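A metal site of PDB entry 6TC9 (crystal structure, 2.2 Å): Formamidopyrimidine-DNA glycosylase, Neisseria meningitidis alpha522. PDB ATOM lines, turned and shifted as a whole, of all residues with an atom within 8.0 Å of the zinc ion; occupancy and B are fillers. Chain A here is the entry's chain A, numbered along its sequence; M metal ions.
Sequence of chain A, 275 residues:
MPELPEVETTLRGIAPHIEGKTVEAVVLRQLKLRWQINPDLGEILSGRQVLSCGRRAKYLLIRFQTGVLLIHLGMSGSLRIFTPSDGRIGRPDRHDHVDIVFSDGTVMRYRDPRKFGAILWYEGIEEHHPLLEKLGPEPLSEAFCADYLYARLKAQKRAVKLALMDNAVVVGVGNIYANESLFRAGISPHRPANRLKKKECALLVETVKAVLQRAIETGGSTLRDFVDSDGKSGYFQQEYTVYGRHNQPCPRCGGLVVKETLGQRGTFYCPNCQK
The side-chain sulfur of Cys 253 sits close to the backbone NH of Gly 255 (3.3 Å). SG of Cys 250 sits close to N of Arg 252, 3.4 Å away. O of Gly 255 sits at hydrogen-bond distance from N of Cys 250, 2.6 Å away. NH1 of Arg 252 lies close to SG of Cys 273 (3.6 Å). The side-chain sulfur (SG) of Cys 270 sits close to the backbone NH (N) of Asn 272 (3.4 Å). The side-chain amide oxygen of Gln 274 lies within hydrogen-bond range of the backbone NH of Cys 270 (3.0 Å).
Of the 18 residues printed, 4 come within 4 Å of the zinc ion. Along chain A the residues within 4 Å of the zinc ion span positions 250 to 273.
SG of Cys 253 is bound to the zinc ion, at 2.2 Å. The side-chain sulfur (SG) of Cys 250 is bound to the zinc ion (2.3 Å). SG of Cys 273 is bound to the zinc ion (2.3 Å). The side-chain sulfur (SG) of Cys 270 is bound to the zinc ion. The zinc ion has four donor atoms within binding distance.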
ATOM      1  N   PHE A 183      -4.301   6.724  23.588  1.00  0.00           N
ATOM      2  CA  PHE A 183      -3.999   8.072  23.098  1.00  0.00           C
ATOM      3  C   PHE A 183      -4.148   9.104  24.212  1.00  0.00           C
ATOM      4  O   PHE A 183      -3.285   9.972  24.404  1.00  0.00           O
ATOM      5  CB  PHE A 183      -4.897   8.448  21.918  1.00  0.00           C
ATOM      6  CG  PHE A 183      -4.802   9.910  21.570  1.00  0.00           C
ATOM      7  CD1 PHE A 183      -3.786  10.363  20.771  1.00  0.00           C
ATOM      8  CD2 PHE A 183      -5.682  10.824  22.104  1.00  0.00           C
ATOM      9  CE1 PHE A 183      -3.665  11.713  20.479  1.00  0.00           C
ATOM     10  CE2 PHE A 183      -5.578  12.158  21.804  1.00  0.00           C
ATOM     11  CZ  PHE A 183      -4.563  12.603  21.000  1.00  0.00           C
ATOM     12  N   THR A 241     -10.751  10.630  19.246  1.00  0.00           N
ATOM     13  CA  THR A 241      -9.469  11.299  19.074  1.00  0.00           C
ATOM     14  C   THR A 241      -8.584  10.559  18.071  1.00  0.00           C
ATOM     15  O   THR A 241      -7.819  11.205  17.339  1.00  0.00           O
ATOM     16  CB  THR A 241      -8.738  11.402  20.425  1.00  0.00           C
ATOM     17  OG1 THR A 241      -8.663  10.095  21.018  1.00  0.00           O
ATOM     18  CG2 THR A 241      -9.460  12.361  21.378  1.00  0.00           C
ATOM     19  N   VAL A 242      -8.626   9.227  18.045  1.00  0.00           N
ATOM     20  CA  VAL A 242      -7.797   8.502  17.093  1.00  0.00           C
ATOM     21  C   VAL A 242      -8.595   7.400  16.415  1.00  0.00           C
ATOM     22  O   VAL A 242      -8.253   6.989  15.299  1.00  0.00           O
ATOM     23  CB  VAL A 242      -6.533   7.889  17.733  1.00  0.00           C
ATOM     24  CG1 VAL A 242      -5.491   8.963  18.070  1.00  0.00           C
ATOM     25  CG2 VAL A 242      -6.851   6.984  18.971  1.00  0.00           C
ATOM     26  N   PRO A 249      -6.073  14.484  10.968  1.00  0.00           N
ATOM     27  CA  PRO A 249      -5.144  15.152  11.900  1.00  0.00           C
ATOM     28  C   PRO A 249      -5.375  14.757  13.357  1.00  0.00           C
ATOM     29  O   PRO A 249      -6.508  14.593  13.806  1.00  0.00           O
ATOM     30  CB  PRO A 249      -5.448  16.637  11.702  1.00  0.00           C
ATOM     31  CG  PRO A 249      -6.874  16.662  11.211  1.00  0.00           C
ATOM     32  CD  PRO A 249      -6.985  15.444  10.329  1.00  0.00           C
ATOM     33  N   CYS A 250      -4.270  14.620  14.064  1.00  0.00           N
ATOM     34  CA  CYS A 250      -4.328  14.376  15.510  1.00  0.00           C
ATOM     35  C   CYS A 250      -4.881  15.627  16.204  1.00  0.00           C
ATOM     36  O   CYS A 250      -4.496  16.735  15.846  1.00  0.00           O
ATOM     37  CB  CYS A 250      -2.932  14.016  16.043  1.00  0.00           C
ATOM     38  SG  CYS A 250      -2.682  14.101  17.866  1.00  0.00           S
ATOM     39  N   PRO A 251      -5.835  15.462  17.131  1.00  0.00           N
ATOM     40  CA  PRO A 251      -6.417  16.661  17.757  1.00  0.00           C
ATOM     41  C   PRO A 251      -5.465  17.427  18.669  1.00  0.00           C
ATOM     42  O   PRO A 251      -5.798  18.542  19.085  1.00  0.00           O
ATOM     43  CB  PRO A 251      -7.581  16.083  18.575  1.00  0.00           C
ATOM     44  CG  PRO A 251      -7.130  14.681  18.900  1.00  0.00           C
ATOM     45  CD  PRO A 251      -6.310  14.213  17.720  1.00  0.00           C
ATOM     46  N   ARG A 252      -4.278  16.887  18.949  1.00  0.00           N
ATOM     47  CA  ARG A 252      -3.335  17.498  19.877  1.00  0.00           C
ATOM     48  C   ARG A 252      -2.193  18.180  19.150  1.00  0.00           C
ATOM     49  O   ARG A 252      -1.887  19.345  19.426  1.00  0.00           O
ATOM     50  CB  ARG A 252      -2.824  16.427  20.860  1.00  0.00           C
ATOM     51  CG  ARG A 252      -1.898  16.949  21.965  1.00  0.00           C
ATOM     52  CD  ARG A 252      -1.429  15.824  22.909  1.00  0.00           C
ATOM     53  NE  ARG A 252      -0.668  16.305  24.072  1.00  0.00           N
ATOM     54  CZ  ARG A 252       0.657  16.464  24.083  1.00  0.00           C
ATOM     55  NH1 ARG A 252       1.377  16.193  23.009  1.00  0.00           N
ATOM     56  NH2 ARG A 252       1.258  16.910  25.182  1.00  0.00           N
ATOM     57  N   CYS A 253      -1.460  17.448  18.305  1.00  0.00           N
ATOM     58  CA  CYS A 253      -0.338  17.985  17.534  1.00  0.00           C
ATOM     59  C   CYS A 253      -0.705  18.400  16.112  1.00  0.00           C
ATOM     60  O   CYS A 253       0.117  19.048  15.450  1.00  0.00           O
ATOM     61  CB  CYS A 253       0.831  17.001  17.492  1.00  0.00           C
ATOM     62  SG  CYS A 253       0.566  15.470  16.620  1.00  0.00           S
ATOM     63  N   GLY A 254      -1.832  17.931  15.573  1.00  0.00           N
ATOM     64  CA  GLY A 254      -2.154  18.122  14.178  1.00  0.00           C
ATOM     65  C   GLY A 254      -1.528  17.139  13.211  1.00  0.00           C
ATOM     66  O   GLY A 254      -1.912  17.128  12.026  1.00  0.00           O
ATOM     67  N   GLY A 255      -0.586  16.312  13.673  1.00  0.00           N
ATOM     68  CA  GLY A 255       0.028  15.308  12.815  1.00  0.00           C
ATOM     69  C   GLY A 255      -0.934  14.192  12.448  1.00  0.00           C
ATOM     70  O   GLY A 255      -1.993  14.008  13.046  1.00  0.00           O
ATOM     71  N   LEU A 256      -0.555  13.418  11.431  1.00  0.00           N
ATOM     72  CA  LEU A 256      -1.467  12.426  10.877  1.00  0.00           C
ATOM     73  C   LEU A 256      -1.523  11.186  11.771  1.00  0.00           C
ATOM     74  O   LEU A 256      -0.485  10.662  12.212  1.00  0.00           O
ATOM     75  CB  LEU A 256      -1.048  12.019   9.469  1.00  0.00           C
ATOM     76  CG  LEU A 256      -0.980  13.082   8.367  1.00  0.00           C
ATOM     77  CD1 LEU A 256       0.261  12.878   7.502  1.00  0.00           C
ATOM     78  CD2 LEU A 256      -2.251  13.057   7.515  1.00  0.00           C
ATOM     79  N   VAL A 257      -2.728  10.699  11.987  1.00  0.00           N
ATOM     80  CA  VAL A 257      -2.947   9.511  12.781  1.00  0.00           C
ATOM     81  C   VAL A 257      -2.613   8.305  11.930  1.00  0.00           C
ATOM     82  O   VAL A 257      -3.046   8.208  10.768  1.00  0.00           O
ATOM     83  CB  VAL A 257      -4.397   9.474  13.291  1.00  0.00           C
ATOM     84  CG1 VAL A 257      -4.697   8.160  13.957  1.00  0.00           C
ATOM     85  CG2 VAL A 257      -4.647  10.628  14.242  1.00  0.00           C
ATOM     86  N   TYR A 269      -3.050   5.449  16.344  1.00  0.00           N
ATOM     87  CA  TYR A 269      -2.395   6.299  17.328  1.00  0.00           C
ATOM     88  C   TYR A 269      -1.586   7.383  16.638  1.00  0.00           C
ATOM     89  O   TYR A 269      -1.234   7.274  15.462  1.00  0.00           O
ATOM     90  CB  TYR A 269      -1.503   5.472  18.262  1.00  0.00           C
ATOM     91  CG  TYR A 269      -0.321   4.841  17.581  1.00  0.00           C
ATOM     92  CD1 TYR A 269       0.975   5.308  17.793  1.00  0.00           C
ATOM     93  CD2 TYR A 269      -0.493   3.749  16.734  1.00  0.00           C
ATOM     94  CE1 TYR A 269       2.067   4.704  17.172  1.00  0.00           C
ATOM     95  CE2 TYR A 269       0.585   3.147  16.113  1.00  0.00           C
ATOM     96  CZ  TYR A 269       1.861   3.623  16.336  1.00  0.00           C
ATOM     97  OH  TYR A 269       2.921   2.996  15.701  1.00  0.00           O
ATOM     98  N   CYS A 270      -1.160   8.356  17.448  1.00  0.00           N
ATOM     99  CA  CYS A 270      -0.235   9.379  16.977  1.00  0.00           C
ATOM    100  C   CYS A 270       1.152   9.103  17.544  1.00  0.00           C
ATOM    101  O   CYS A 270       1.332   9.140  18.780  1.00  0.00           O
ATOM    102  CB  CYS A 270      -0.707  10.763  17.413  1.00  0.00           C
ATOM    103  SG  CYS A 270       0.516  12.028  17.115  1.00  0.00           S
ATOM    104  N   PRO A 271       2.159   8.864  16.703  1.00  0.00           N
ATOM    105  CA  PRO A 271       3.487   8.523  17.240  1.00  0.00           C
ATOM    106  C   PRO A 271       4.191   9.708  17.849  1.00  0.00           C
ATOM    107  O   PRO A 271       5.243   9.539  18.479  1.00  0.00           O
ATOM    108  CB  PRO A 271       4.241   7.983  16.017  1.00  0.00           C
ATOM    109  CG  PRO A 271       3.448   8.301  14.834  1.00  0.00           C
ATOM    110  CD  PRO A 271       2.058   8.704  15.245  1.00  0.00           C
ATOM    111  N   ASN A 272       3.629  10.905  17.688  1.00  0.00           N
ATOM    112  CA  ASN A 272       4.194  12.115  18.265  1.00  0.00           C
ATOM    113  C   ASN A 272       3.718  12.334  19.700  1.00  0.00           C
ATOM    114  O   ASN A 272       4.522  12.681  20.562  1.00  0.00           O
ATOM    115  CB  ASN A 272       3.844  13.320  17.396  1.00  0.00           C
ATOM    116  CG  ASN A 272       4.650  14.539  17.737  1.00  0.00           C
ATOM    117  OD1 ASN A 272       5.805  14.667  17.351  1.00  0.00           O
ATOM    118  ND2 ASN A 272       4.033  15.465  18.484  1.00  0.00           N
ATOM    119  N   CYS A 273       2.440  12.087  19.976  1.00  0.00           N
ATOM    120  CA  CYS A 273       1.897  12.317  21.300  1.00  0.00           C
ATOM    121  C   CYS A 273       1.820  11.028  22.119  1.00  0.00           C
ATOM    122  O   CYS A 273       1.263  11.045  23.222  1.00  0.00           O
ATOM    123  CB  CYS A 273       0.495  12.926  21.186  1.00  0.00           C
ATOM    124  SG  CYS A 273       0.295  14.400  20.109  1.00  0.00           S
ATOM    125  N   GLN A 274       2.399   9.925  21.636  1.00  0.00           N
ATOM    126  CA  GLN A 274       2.317   8.629  22.317  1.00  0.00           C
ATOM    127  C   GLN A 274       3.644   7.924  22.176  1.00  0.00           C
ATOM    128  O   GLN A 274       4.071   7.653  21.051  1.00  0.00           O
ATOM    129  CB  GLN A 274       1.203   7.764  21.705  1.00  0.00           C
ATOM    130  CG  GLN A 274      -0.190   8.271  21.939  1.00  0.00           C
ATOM    131  CD  GLN A 274      -1.265   7.421  21.267  1.00  0.00           C
ATOM    132  OE1 GLN A 274      -1.901   7.854  20.300  1.00  0.00           O
ATOM    133  NE2 GLN A 274      -1.483   6.211  21.796  1.00  0.00           N
HETATM  134 ZN    ZN M   1      -0.411  13.997  17.972  1.00  0.00          ZN
